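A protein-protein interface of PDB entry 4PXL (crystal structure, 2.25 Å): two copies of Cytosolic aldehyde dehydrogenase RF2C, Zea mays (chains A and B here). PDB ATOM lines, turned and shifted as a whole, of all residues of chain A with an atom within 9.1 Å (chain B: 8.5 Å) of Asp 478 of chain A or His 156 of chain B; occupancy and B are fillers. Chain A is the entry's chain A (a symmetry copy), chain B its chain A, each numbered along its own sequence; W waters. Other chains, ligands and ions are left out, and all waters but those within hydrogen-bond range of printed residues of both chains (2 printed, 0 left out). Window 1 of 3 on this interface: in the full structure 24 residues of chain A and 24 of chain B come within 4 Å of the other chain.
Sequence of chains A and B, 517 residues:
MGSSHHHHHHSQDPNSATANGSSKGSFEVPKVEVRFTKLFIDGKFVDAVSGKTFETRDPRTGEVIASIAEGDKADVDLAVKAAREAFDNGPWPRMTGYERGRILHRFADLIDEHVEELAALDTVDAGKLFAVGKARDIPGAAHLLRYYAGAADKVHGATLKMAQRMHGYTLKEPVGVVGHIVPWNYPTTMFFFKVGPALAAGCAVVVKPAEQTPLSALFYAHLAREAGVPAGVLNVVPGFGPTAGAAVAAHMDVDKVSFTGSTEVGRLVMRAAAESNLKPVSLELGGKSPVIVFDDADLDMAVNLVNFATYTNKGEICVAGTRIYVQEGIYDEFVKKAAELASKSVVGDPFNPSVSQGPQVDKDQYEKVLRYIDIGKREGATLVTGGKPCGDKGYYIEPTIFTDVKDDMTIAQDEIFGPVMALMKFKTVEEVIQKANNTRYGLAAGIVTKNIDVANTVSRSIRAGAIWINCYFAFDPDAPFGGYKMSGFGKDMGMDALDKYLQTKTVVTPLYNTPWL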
ATOM      1  N   HIS A 143     -31.966 -37.276  18.959  1.00  0.00           N
ATOM      2  CA  HIS A 143     -30.871 -36.321  18.717  1.00  0.00           C
ATOM      3  C   HIS A 143     -30.970 -35.746  17.277  1.00  0.00           C
ATOM      4  O   HIS A 143     -30.883 -34.535  17.097  1.00  0.00           O
ATOM      5  CB  HIS A 143     -29.505 -37.019  18.948  1.00  0.00           C
ATOM      6  CG  HIS A 143     -28.282 -36.227  18.566  1.00  0.00           C
ATOM      7  ND1 HIS A 143     -27.011 -36.712  18.828  1.00  0.00           N
ATOM      8  CD2 HIS A 143     -28.162 -35.012  17.966  1.00  0.00           C
ATOM      9  CE1 HIS A 143     -26.172 -35.794  18.379  1.00  0.00           C
ATOM     10  NE2 HIS A 143     -26.814 -34.753  17.862  1.00  0.00           N
ATOM     11  N   LEU A 144     -31.152 -36.614  16.258  1.00  0.00           N
ATOM     12  CA  LEU A 144     -31.266 -36.172  14.862  1.00  0.00           C
ATOM     13  C   LEU A 144     -32.511 -35.311  14.683  1.00  0.00           C
ATOM     14  O   LEU A 144     -32.497 -34.368  13.894  1.00  0.00           O
ATOM     15  CB  LEU A 144     -31.282 -37.382  13.893  1.00  0.00           C
ATOM     16  CG  LEU A 144     -31.439 -37.047  12.398  1.00  0.00           C
ATOM     17  CD1 LEU A 144     -30.114 -36.742  11.731  1.00  0.00           C
ATOM     18  CD2 LEU A 144     -32.104 -38.136  11.671  1.00  0.00           C
ATOM     19  N   TYR A 147     -31.646 -31.848  15.984  1.00  0.00           N
ATOM     20  CA  TYR A 147     -30.827 -31.156  14.982  1.00  0.00           C
ATOM     21  C   TYR A 147     -31.749 -30.392  13.971  1.00  0.00           C
ATOM     22  O   TYR A 147     -31.554 -29.207  13.760  1.00  0.00           O
ATOM     23  CB  TYR A 147     -29.905 -32.147  14.273  1.00  0.00           C
ATOM     24  CG  TYR A 147     -29.053 -31.521  13.193  1.00  0.00           C
ATOM     25  CD1 TYR A 147     -27.840 -30.927  13.496  1.00  0.00           C
ATOM     26  CD2 TYR A 147     -29.470 -31.505  11.870  1.00  0.00           C
ATOM     27  CE1 TYR A 147     -27.061 -30.333  12.506  1.00  0.00           C
ATOM     28  CE2 TYR A 147     -28.673 -30.959  10.866  1.00  0.00           C
ATOM     29  CZ  TYR A 147     -27.476 -30.364  11.193  1.00  0.00           C
ATOM     30  OH  TYR A 147     -26.727 -29.795  10.206  1.00  0.00           O
ATOM     31  N   TYR A 148     -32.778 -31.051  13.424  1.00  0.00           N
ATOM     32  CA  TYR A 148     -33.707 -30.410  12.477  1.00  0.00           C
ATOM     33  C   TYR A 148     -34.657 -29.460  13.108  1.00  0.00           C
ATOM     34  O   TYR A 148     -34.952 -28.443  12.504  1.00  0.00           O
ATOM     35  CB  TYR A 148     -34.429 -31.433  11.591  1.00  0.00           C
ATOM     36  CG  TYR A 148     -33.444 -32.097  10.671  1.00  0.00           C
ATOM     37  CD1 TYR A 148     -32.840 -31.382   9.634  1.00  0.00           C
ATOM     38  CD2 TYR A 148     -32.993 -33.396  10.921  1.00  0.00           C
ATOM     39  CE1 TYR A 148     -31.836 -31.958   8.848  1.00  0.00           C
ATOM     40  CE2 TYR A 148     -31.992 -33.978  10.142  1.00  0.00           C
ATOM     41  CZ  TYR A 148     -31.417 -33.252   9.114  1.00  0.00           C
ATOM     42  OH  TYR A 148     -30.461 -33.824   8.333  1.00  0.00           O
ATOM     43  N   ALA A 151     -32.872 -26.346  13.220  1.00  0.00           N
ATOM     44  CA  ALA A 151     -32.637 -25.780  11.881  1.00  0.00           C
ATOM     45  C   ALA A 151     -33.875 -25.072  11.365  1.00  0.00           C
ATOM     46  O   ALA A 151     -33.769 -24.209  10.490  1.00  0.00           O
ATOM     47  CB  ALA A 151     -32.270 -26.898  10.905  1.00  0.00           C
ATOM     48  N   ALA A 474     -19.051 -43.170  11.117  1.00  0.00           N
ATOM     49  CA  ALA A 474     -18.966 -41.853  11.749  1.00  0.00           C
ATOM     50  C   ALA A 474     -20.088 -40.944  11.234  1.00  0.00           C
ATOM     51  O   ALA A 474     -19.849 -39.862  10.711  1.00  0.00           O
ATOM     52  CB  ALA A 474     -17.580 -41.240  11.514  1.00  0.00           C
ATOM     53  N   PHE A 475     -21.329 -41.417  11.390  1.00  0.00           N
ATOM     54  CA  PHE A 475     -22.521 -40.657  11.017  1.00  0.00           C
ATOM     55  C   PHE A 475     -22.679 -39.573  12.053  1.00  0.00           C
ATOM     56  O   PHE A 475     -22.307 -39.759  13.202  1.00  0.00           O
ATOM     57  CB  PHE A 475     -23.791 -41.533  11.041  1.00  0.00           C
ATOM     58  CG  PHE A 475     -23.815 -42.624  10.010  1.00  0.00           C
ATOM     59  CD1 PHE A 475     -24.135 -42.344   8.684  1.00  0.00           C
ATOM     60  CD2 PHE A 475     -23.551 -43.940  10.363  1.00  0.00           C
ATOM     61  CE1 PHE A 475     -24.162 -43.365   7.725  1.00  0.00           C
ATOM     62  CE2 PHE A 475     -23.573 -44.960   9.397  1.00  0.00           C
ATOM     63  CZ  PHE A 475     -23.883 -44.665   8.089  1.00  0.00           C
ATOM     64  N   ASP A 476     -23.245 -38.444  11.652  1.00  0.00           N
ATOM     65  CA  ASP A 476     -23.498 -37.340  12.556  1.00  0.00           C
ATOM     66  C   ASP A 476     -24.658 -36.546  11.998  1.00  0.00           C
ATOM     67  O   ASP A 476     -24.684 -36.298  10.789  1.00  0.00           O
ATOM     68  CB  ASP A 476     -22.256 -36.444  12.674  1.00  0.00           C
ATOM     69  CG  ASP A 476     -22.347 -35.455  13.815  1.00  0.00           C
ATOM     70  OD1 ASP A 476     -22.970 -34.382  13.627  1.00  0.00           O
ATOM     71  OD2 ASP A 476     -21.867 -35.778  14.916  1.00  0.00           O
ATOM     72  N   PRO A 477     -25.597 -36.071  12.843  1.00  0.00           N
ATOM     73  CA  PRO A 477     -26.684 -35.229  12.309  1.00  0.00           C
ATOM     74  C   PRO A 477     -26.203 -34.086  11.399  1.00  0.00           C
ATOM     75  O   PRO A 477     -26.909 -33.761  10.451  1.00  0.00           O
ATOM     76  CB  PRO A 477     -27.388 -34.730  13.564  1.00  0.00           C
ATOM     77  CG  PRO A 477     -27.150 -35.839  14.566  1.00  0.00           C
ATOM     78  CD  PRO A 477     -25.751 -36.281  14.305  1.00  0.00           C
ATOM     79  N   ASP A 478     -25.008 -33.511  11.656  1.00  0.00           N
ATOM     80  CA  ASP A 478     -24.458 -32.390  10.873  1.00  0.00           C
ATOM     81  C   ASP A 478     -23.735 -32.787   9.571  1.00  0.00           C
ATOM     82  O   ASP A 478     -23.437 -31.922   8.735  1.00  0.00           O
ATOM     83  CB  ASP A 478     -23.576 -31.459  11.744  1.00  0.00           C
ATOM     84  CG  ASP A 478     -23.287 -30.086  11.104  1.00  0.00           C
ATOM     85  OD1 ASP A 478     -24.244 -29.455  10.565  1.00  0.00           O
ATOM     86  OD2 ASP A 478     -22.114 -29.651  11.123  1.00  0.00           O
ATOM     87  N   ALA A 479     -23.481 -34.084   9.395  1.00  0.00           N
ATOM     88  CA  ALA A 479     -22.737 -34.595   8.249  1.00  0.00           C
ATOM     89  C   ALA A 479     -23.643 -35.213   7.177  1.00  0.00           C
ATOM     90  O   ALA A 479     -24.326 -36.209   7.455  1.00  0.00           O
ATOM     91  CB  ALA A 479     -21.673 -35.603   8.713  1.00  0.00           C
ATOM     92  N   PRO A 480     -23.661 -34.639   5.939  1.00  0.00           N
ATOM     93  CA  PRO A 480     -24.483 -35.247   4.867  1.00  0.00           C
ATOM     94  C   PRO A 480     -23.997 -36.638   4.499  1.00  0.00           C
ATOM     95  O   PRO A 480     -22.786 -36.899   4.497  1.00  0.00           O
ATOM     96  CB  PRO A 480     -24.325 -34.291   3.675  1.00  0.00           C
ATOM     97  CG  PRO A 480     -23.132 -33.449   3.974  1.00  0.00           C
ATOM     98  CD  PRO A 480     -22.921 -33.448   5.460  1.00  0.00           C
ATOM     99  N   PHE A 481     -24.936 -37.528   4.195  1.00  0.00           N
ATOM    100  CA  PHE A 481     -24.644 -38.904   3.848  1.00  0.00           C
ATOM    101  C   PHE A 481     -25.412 -39.293   2.591  1.00  0.00           C
ATOM    102  O   PHE A 481     -26.631 -39.163   2.537  1.00  0.00           O
ATOM    103  CB  PHE A 481     -25.008 -39.818   5.027  1.00  0.00           C
ATOM    104  CG  PHE A 481     -24.856 -41.279   4.699  1.00  0.00           C
ATOM    105  CD1 PHE A 481     -23.590 -41.856   4.582  1.00  0.00           C
ATOM    106  CD2 PHE A 481     -25.975 -42.068   4.424  1.00  0.00           C
ATOM    107  CE1 PHE A 481     -23.451 -43.203   4.236  1.00  0.00           C
ATOM    108  CE2 PHE A 481     -25.826 -43.401   4.037  1.00  0.00           C
ATOM    109  CZ  PHE A 481     -24.570 -43.963   3.987  1.00  0.00           C
ATOM    110  N   ASP A 492     -28.988 -37.742   3.033  1.00  0.00           N
ATOM    111  CA  ASP A 492     -29.707 -37.895   4.289  1.00  0.00           C
ATOM    112  C   ASP A 492     -28.724 -37.323   5.300  1.00  0.00           C
ATOM    113  O   ASP A 492     -27.503 -37.418   5.082  1.00  0.00           O
ATOM    114  CB  ASP A 492     -30.019 -39.362   4.602  1.00  0.00           C
ATOM    115  CG  ASP A 492     -31.231 -39.924   3.869  1.00  0.00           C
ATOM    116  OD1 ASP A 492     -32.210 -39.165   3.654  1.00  0.00           O
ATOM    117  OD2 ASP A 492     -31.195 -41.113   3.500  1.00  0.00           O
ATOM    118  N   MET A 493     -29.232 -36.712   6.392  1.00  0.00           N
ATOM    119  CA  MET A 493     -28.392 -36.071   7.424  1.00  0.00           C
ATOM    120  C   MET A 493     -27.758 -34.762   6.911  1.00  0.00           C
ATOM    121  O   MET A 493     -27.720 -34.499   5.700  1.00  0.00           O
ATOM    122  CB  MET A 493     -27.362 -37.034   8.050  1.00  0.00           C
ATOM    123  CG  MET A 493     -27.997 -38.281   8.615  1.00  0.00           C
ATOM    124  SD  MET A 493     -26.807 -39.444   9.315  1.00  0.00           S
ATOM    125  CE  MET A 493     -27.053 -39.088  11.079  1.00  0.00           C
ATOM    126  N   GLY A 494     -27.340 -33.918   7.850  1.00  0.00           N
ATOM    127  CA  GLY A 494     -26.775 -32.610   7.543  1.00  0.00           C
ATOM    128  C   GLY A 494     -27.846 -31.619   7.116  1.00  0.00           C
ATOM    129  O   GLY A 494     -29.038 -31.938   7.034  1.00  0.00           O
ATOM    130  N   MET A 495     -27.423 -30.413   6.827  1.00  0.00           N
ATOM    131  CA  MET A 495     -28.305 -29.360   6.320  1.00  0.00           C
ATOM    132  C   MET A 495     -28.785 -29.729   4.903  1.00  0.00           C
ATOM    133  O   MET A 495     -29.829 -29.266   4.483  1.00  0.00           O
ATOM    134  CB  MET A 495     -27.566 -27.997   6.304  1.00  0.00           C
ATOM    135  CG  MET A 495     -27.220 -27.445   7.687  1.00  0.00           C
ATOM    136  SD  MET A 495     -28.617 -27.309   8.844  1.00  0.00           S
ATOM    137  CE  MET A 495     -29.608 -26.003   8.041  1.00  0.00           C
ATOM    138  N   ASP A 496     -28.016 -30.558   4.176  1.00  0.00           N
ATOM    139  CA  ASP A 496     -28.339 -31.038   2.810  1.00  0.00           C
ATOM    140  C   ASP A 496     -29.676 -31.765   2.757  1.00  0.00           C
ATOM    141  O   ASP A 496     -30.413 -31.585   1.790  1.00  0.00           O
ATOM    142  CB  ASP A 496     -27.226 -31.951   2.264  1.00  0.00           C
ATOM    143  CG  ASP A 496     -25.828 -31.348   2.338  1.00  0.00           C
ATOM    144  OD1 ASP A 496     -25.410 -30.926   3.462  1.00  0.00           O
ATOM    145  OD2 ASP A 496     -25.138 -31.321   1.290  1.00  0.00           O
ATOM    146  N   ALA A 497     -29.990 -32.579   3.794  1.00  0.00           N
ATOM    147  CA  ALA A 497     -31.242 -33.331   3.877  1.00  0.00           C
ATOM    148  C   ALA A 497     -32.424 -32.349   3.998  1.00  0.00           C
ATOM    149  O   ALA A 497     -33.449 -32.559   3.354  1.00  0.00           O
ATOM    150  CB  ALA A 497     -31.224 -34.288   5.064  1.00  0.00           C
ATOM    151  N   GLY B 150     -30.075 -24.009  19.157  1.00  0.00           N
ATOM    152  CA  GLY B 150     -30.288 -24.740  17.908  1.00  0.00           C
ATOM    153  C   GLY B 150     -29.213 -24.519  16.858  1.00  0.00           C
ATOM    154  O   GLY B 150     -29.086 -25.326  15.936  1.00  0.00           O
ATOM    155  N   ALA B 151     -28.409 -23.444  16.995  1.00  0.00           N
ATOM    156  CA  ALA B 151     -27.309 -23.121  16.071  1.00  0.00           C
ATOM    157  C   ALA B 151     -26.021 -23.795  16.502  1.00  0.00           C
ATOM    158  O   ALA B 151     -25.124 -23.991  15.678  1.00  0.00           O
ATOM    159  CB  ALA B 151     -27.083 -21.609  16.044  1.00  0.00           C
ATOM    160  N   ALA B 152     -25.925 -24.129  17.796  1.00  0.00           N
ATOM    161  CA  ALA B 152     -24.729 -24.656  18.442  1.00  0.00           C
ATOM    162  C   ALA B 152     -24.121 -25.885  17.819  1.00  0.00           C
ATOM    163  O   ALA B 152     -22.895 -25.968  17.754  1.00  0.00           O
ATOM    164  CB  ALA B 152     -24.961 -24.855  19.932  1.00  0.00           C
ATOM    165  N   ASP B 153     -24.954 -26.795  17.288  1.00  0.00           N
ATOM    166  CA  ASP B 153     -24.477 -28.035  16.690  1.00  0.00           C
ATOM    167  C   ASP B 153     -24.385 -28.017  15.136  1.00  0.00           C
ATOM    168  O   ASP B 153     -24.209 -29.074  14.532  1.00  0.00           O
ATOM    169  CB  ASP B 153     -25.366 -29.186  17.197  1.00  0.00           C
ATOM    170  CG  ASP B 153     -26.785 -29.226  16.652  1.00  0.00           C
ATOM    171  OD1 ASP B 153     -27.191 -28.252  15.968  1.00  0.00           O
ATOM    172  OD2 ASP B 153     -27.487 -30.267  16.876  1.00  0.00           O
ATOM    173  N   LYS B 154     -24.499 -26.816  14.523  1.00  0.00           N
ATOM    174  CA  LYS B 154     -24.589 -26.537  13.088  1.00  0.00           C
ATOM    175  C   LYS B 154     -23.586 -25.500  12.601  1.00  0.00           C
ATOM    176  O   LYS B 154     -23.765 -24.972  11.500  1.00  0.00           O
ATOM    177  CB  LYS B 154     -25.953 -25.883  12.841  1.00  0.00           C
ATOM    178  CG  LYS B 154     -27.021 -26.843  12.607  1.00  0.00           C
ATOM    179  CD  LYS B 154     -28.355 -26.197  12.741  1.00  0.00           C
ATOM    180  CE  LYS B 154     -29.301 -27.349  13.018  1.00  0.00           C
ATOM    181  NZ  LYS B 154     -29.399 -27.646  14.487  1.00  0.00           N
ATOM    182  N   VAL B 155     -22.599 -25.127  13.434  1.00  0.00           N
ATOM    183  CA  VAL B 155     -21.614 -24.113  13.099  1.00  0.00           C
ATOM    184  C   VAL B 155     -20.698 -24.683  12.003  1.00  0.00           C
ATOM    185  O   VAL B 155     -20.096 -25.727  12.203  1.00  0.00           O
ATOM    186  CB  VAL B 155     -20.805 -23.721  14.385  1.00  0.00           C
ATOM    187  CG1 VAL B 155     -19.611 -22.841  14.042  1.00  0.00           C
ATOM    188  CG2 VAL B 155     -21.690 -23.055  15.437  1.00  0.00           C
ATOM    189  N   HIS B 156     -20.576 -23.999  10.867  1.00  0.00           N
ATOM    190  CA  HIS B 156     -19.701 -24.497   9.807  1.00  0.00           C
ATOM    191  C   HIS B 156     -18.636 -23.523   9.397  1.00  0.00           C
ATOM    192  O   HIS B 156     -18.904 -22.343   9.246  1.00  0.00           O
ATOM    193  CB  HIS B 156     -20.486 -24.813   8.513  1.00  0.00           C
ATOM    194  CG  HIS B 156     -21.537 -25.874   8.616  1.00  0.00           C
ATOM    195  ND1 HIS B 156     -22.421 -26.115   7.559  1.00  0.00           N
ATOM    196  CD2 HIS B 156     -21.834 -26.717   9.633  1.00  0.00           C
ATOM    197  CE1 HIS B 156     -23.205 -27.093   7.971  1.00  0.00           C
ATOM    198  NE2 HIS B 156     -22.906 -27.474   9.213  1.00  0.00           N
ATOM    199  N   GLY B 157     -17.465 -24.064   9.085  1.00  0.00           N
ATOM    200  CA  GLY B 157     -16.399 -23.349   8.409  1.00  0.00           C
ATOM    201  C   GLY B 157     -16.480 -23.782   6.950  1.00  0.00           C
ATOM    202  O   GLY B 157     -17.511 -24.309   6.510  1.00  0.00           O
ATOM    203  N   ALA B 158     -15.408 -23.590   6.188  1.00  0.00           N
ATOM    204  CA  ALA B 158     -15.381 -23.932   4.768  1.00  0.00           C
ATOM    205  C   ALA B 158     -14.201 -24.802   4.363  1.00  0.00           C
ATOM    206  O   ALA B 158     -13.127 -24.667   4.924  1.00  0.00           O
ATOM    207  CB  ALA B 158     -15.332 -22.645   3.949  1.00  0.00           C
ATOM    208  N   THR B 159     -14.364 -25.616   3.307  1.00  0.00           N
ATOM    209  CA  THR B 159     -13.230 -26.278   2.644  1.00  0.00           C
ATOM    210  C   THR B 159     -13.038 -25.389   1.405  1.00  0.00           C
ATOM    211  O   THR B 159     -14.008 -25.016   0.724  1.00  0.00           O
ATOM    212  CB  THR B 159     -13.421 -27.770   2.339  1.00  0.00           C
ATOM    213  OG1 THR B 159     -14.561 -27.944   1.511  1.00  0.00           O
ATOM    214  CG2 THR B 159     -13.487 -28.633   3.603  1.00  0.00           C
ATOM    215  N   THR B 170     -11.173 -23.792   6.638  1.00  0.00           N
ATOM    216  CA  THR B 170     -11.269 -22.897   7.785  1.00  0.00           C
ATOM    217  C   THR B 170     -11.965 -23.595   8.929  1.00  0.00           C
ATOM    218  O   THR B 170     -12.900 -24.359   8.707  1.00  0.00           O
ATOM    219  CB  THR B 170     -11.937 -21.541   7.446  1.00  0.00           C
ATOM    220  OG1 THR B 170     -13.309 -21.758   7.157  1.00  0.00           O
ATOM    221  CG2 THR B 170     -11.239 -20.781   6.311  1.00  0.00           C
ATOM    222  N   LEU B 171     -11.520 -23.328  10.140  1.00  0.00           N
ATOM    223  CA  LEU B 171     -12.131 -23.832  11.382  1.00  0.00           C
ATOM    224  C   LEU B 171     -12.767 -22.671  12.133  1.00  0.00           C
ATOM    225  O   LEU B 171     -12.186 -21.596  12.198  1.00  0.00           O
ATOM    226  CB  LEU B 171     -11.085 -24.519  12.301  1.00  0.00           C
ATOM    227  CG  LEU B 171     -10.431 -25.798  11.771  1.00  0.00           C
ATOM    228  CD1 LEU B 171      -9.322 -26.235  12.688  1.00  0.00           C
ATOM    229  CD2 LEU B 171     -11.462 -26.912  11.571  1.00  0.00           C
ATOM    230  N   LYS B 172     -13.943 -22.891  12.702  1.00  0.00           N
ATOM    231  CA  LYS B 172     -14.630 -21.884  13.499  1.00  0.00           C
ATOM    232  C   LYS B 172     -14.427 -22.202  14.986  1.00  0.00           C
ATOM    233  O   LYS B 172     -14.980 -23.155  15.513  1.00  0.00           O
ATOM    234  CB  LYS B 172     -16.120 -21.798  13.115  1.00  0.00           C
ATOM    235  CG  LYS B 172     -16.337 -21.302  11.693  1.00  0.00           C
ATOM    236  CD  LYS B 172     -16.213 -19.800  11.574  1.00  0.00           C
ATOM    237  CE  LYS B 172     -16.446 -19.383  10.148  1.00  0.00           C
ATOM    238  NZ  LYS B 172     -16.597 -17.913  10.029  1.00  0.00           N
ATOM    239  N   GLU B 173     -13.563 -21.453  15.642  1.00  0.00           N
ATOM    240  CA  GLU B 173     -13.288 -21.723  17.048  1.00  0.00           C
ATOM    241  C   GLU B 173     -13.763 -20.655  18.000  1.00  0.00           C
ATOM    242  O   GLU B 173     -13.805 -19.480  17.617  1.00  0.00           O
ATOM    243  CB  GLU B 173     -11.827 -22.123  17.320  1.00  0.00           C
ATOM    244  CG  GLU B 173     -10.722 -21.534  16.490  1.00  0.00           C
ATOM    245  CD  GLU B 173      -9.376 -22.063  16.977  1.00  0.00           C
ATOM    246  OE1 GLU B 173      -8.847 -21.498  17.964  1.00  0.00           O
ATOM    247  OE2 GLU B 173      -8.892 -23.091  16.437  1.00  0.00           O
ATOM    248  N   MET B 495     -27.565 -15.187  12.725  1.00  0.00           N
ATOM    249  CA  MET B 495     -26.368 -16.031  12.700  1.00  0.00           C
ATOM    250  C   MET B 495     -25.112 -15.145  12.800  1.00  0.00           C
ATOM    251  O   MET B 495     -24.080 -15.615  13.239  1.00  0.00           O
ATOM    252  CB  MET B 495     -26.332 -16.878  11.400  1.00  0.00           C
ATOM    253  CG  MET B 495     -27.433 -17.932  11.298  1.00  0.00           C
ATOM    254  SD  MET B 495     -27.551 -19.077  12.707  1.00  0.00           S
ATOM    255  CE  MET B 495     -25.986 -20.001  12.537  1.00  0.00           C
ATOM    256  N   LEU B 498     -23.637 -14.931  16.298  1.00  0.00           N
ATOM    257  CA  LEU B 498     -22.895 -16.143  16.598  1.00  0.00           C
ATOM    258  C   LEU B 498     -21.498 -16.047  15.994  1.00  0.00           C
ATOM    259  O   LEU B 498     -20.520 -16.231  16.715  1.00  0.00           O
ATOM    260  CB  LEU B 498     -23.648 -17.382  16.085  1.00  0.00           C
ATOM    261  CG  LEU B 498     -23.024 -18.756  16.415  1.00  0.00           C
ATOM    262  CD1 LEU B 498     -22.951 -19.009  17.926  1.00  0.00           C
ATOM    263  CD2 LEU B 498     -23.784 -19.871  15.732  1.00  0.00           C
ATOM    264  N   ASP B 499     -21.403 -15.606  14.714  1.00  0.00           N
ATOM    265  CA  ASP B 499     -20.127 -15.411  14.043  1.00  0.00           C
ATOM    266  C   ASP B 499     -19.141 -14.477  14.758  1.00  0.00           C
ATOM    267  O   ASP B 499     -17.941 -14.681  14.653  1.00  0.00           O
ATOM    268  CB  ASP B 499     -20.284 -15.037  12.556  1.00  0.00           C
ATOM    269  CG  ASP B 499     -18.972 -15.180  11.771  1.00  0.00           C
ATOM    270  OD1 ASP B 499     -18.207 -16.156  12.039  1.00  0.00           O
ATOM    271  OD2 ASP B 499     -18.689 -14.302  10.922  1.00  0.00           O
ATOM    272  N   LEU B 502     -16.864 -16.452  17.241  1.00  0.00           N
ATOM    273  CA  LEU B 502     -16.050 -17.468  16.596  1.00  0.00           C
ATOM    274  C   LEU B 502     -14.884 -16.847  15.842  1.00  0.00           C
ATOM    275  O   LEU B 502     -15.068 -15.909  15.079  1.00  0.00           O
ATOM    276  CB  LEU B 502     -16.913 -18.264  15.588  1.00  0.00           C
ATOM    277  CG  LEU B 502     -18.065 -19.067  16.188  1.00  0.00           C
ATOM    278  CD1 LEU B 502     -19.094 -19.409  15.152  1.00  0.00           C
ATOM    279  CD2 LEU B 502     -17.569 -20.280  16.968  1.00  0.00           C
ATOM    280  N   GLN B 503     -13.696 -17.423  15.982  1.00  0.00           N
ATOM    281  CA  GLN B 503     -12.538 -17.017  15.195  1.00  0.00           C
ATOM    282  C   GLN B 503     -12.576 -17.905  13.954  1.00  0.00           C
ATOM    283  O   GLN B 503     -13.071 -19.020  14.027  1.00  0.00           O
ATOM    284  CB  GLN B 503     -11.242 -17.369  15.938  1.00  0.00           C
ATOM    285  CG  GLN B 503     -11.046 -16.743  17.319  1.00  0.00           C
ATOM    286  CD  GLN B 503     -10.260 -15.461  17.268  1.00  0.00           C
ATOM    287  OE1 GLN B 503     -10.294 -14.693  16.278  1.00  0.00           O
ATOM    288  NE2 GLN B 503      -9.538 -15.202  18.356  1.00  0.00           N
ATOM    289  N   THR B 504     -12.006 -17.438  12.839  1.00  0.00           N
ATOM    290  CA  THR B 504     -11.836 -18.217  11.618  1.00  0.00           C
ATOM    291  C   THR B 504     -10.356 -18.551  11.567  1.00  0.00           C
ATOM    292  O   THR B 504      -9.530 -17.653  11.612  1.00  0.00           O
ATOM    293  CB  THR B 504     -12.272 -17.420  10.385  1.00  0.00           C
ATOM    294  OG1 THR B 504     -13.665 -17.168  10.510  1.00  0.00           O
ATOM    295  CG2 THR B 504     -11.942 -18.142   9.031  1.00  0.00           C
HETATM  296  O   HOH W   1     -26.013 -32.753  16.663  1.00  0.00           O
HETATM  297  O   HOH W   2     -23.829 -31.795  15.527  1.00  0.00           O
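OD1 of Asp 478 of chain A sits at hydrogen-bond distance from NE2 of His 156 of chain B. The side-chain amino group (NZ) of Lys 154 of chain B lies within hydrogen-bond range of the backbone carbonyl oxygen (O) of Tyr 147 of chain A (2.8 Å).
NE2 of His 156 of chain B sits close to O of Lys 154 of chain B, 3.5 Å away. The side-chain carboxylate of Asp 476 of chain A is in hydrogen-bond range of the backbone NH of Asp 478 of chain A (3.0 Å). NZ of Lys 154 of chain B is in salt-bridge range of OD1 of Asp 153 of chain B, 2.7 Å away. O of Gly 150 of chain B sits at hydrogen-bond distance from NZ of Lys 154 of chain B (2.8 Å). OH of Tyr 147 of chain A sits at hydrogen-bond distance from SD of Met 495 of chain A (3.4 Å).
Among the printed residues, merely in contact across the chains: Tyr 147 of chain A with Asp 153 of chain B (3.5 Å), Ala 151 of chain A with Lys 154 of chain B (3.7 Å), Asp 478 of chain A with Asp 153 of chain B (3.7 Å) and Asp 478 of chain A with Lys 154 of chain B (3.9 Å).
Asp 478 of chain A touches just these residues of chain B: Asp 153 (3.7 Å), Lys 154 (3.9 Å) and His 156 (2.7 Å). Of the printed residues of chain A, His 156 of chain B touches Asp 478. Pro 477 of chain A touches none of the printed residues of chain B. Ala 479 of chain A touches none of the printed residues of chain B. No residue of chain A comes within 4 Å of Val 155 of chain B. No residue of chain A comes within 4 Å of Gly 157 of chain B. Printed residues of chain B within 4 Å of Tyr 147 of chain A: Asp 153 and Lys 154. Printed residues of chain B within 4 Å of Ala 151 of chain A: Lys 154. Of the printed residues of chain A, Lys 154 of chain B touches Tyr 147 (2.8 Å), Ala 151 (3.7 Å) and Asp 478 (3.9 Å).
Of the 19 printed residues of chain A, 3 touch a printed residue of chain B. Hydrophobic or aromatic side chains of chain A that line the printed part of chain B: Tyr 147 and Ala 151. Along chain A the printed residues that touch a printed residue of chain B span positions 147 to 478. Printed residues of chain B that touch a printed residue of chain A: Asp 153, Lys 154 and His 156. Hydrophobic or aromatic side chains of chain B that line the printed part of chain A: His 156. Among the printed residues, 6 pairs touch across the chains. Among the printed residues, no Asp or Glu carboxylate lies within 4 Å of a Lys or Arg side-chain nitrogen of the other chain.
2 positions are printed for both chains. Of the 6 pairs that touch across the chains among the printed residues, none has its exchanged pair printed and touching as well.
Water W1 bridges a ring nitrogen (NE2) of His 143 of chain A and the side-chain carboxylate (OD2) of Asp 153 of chain B. Water W2 lies within hydrogen-bond range of O of Asp 153 of chain B (2.9 Å) and OD1 of Asp 476 of chain A (3.3 Å).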
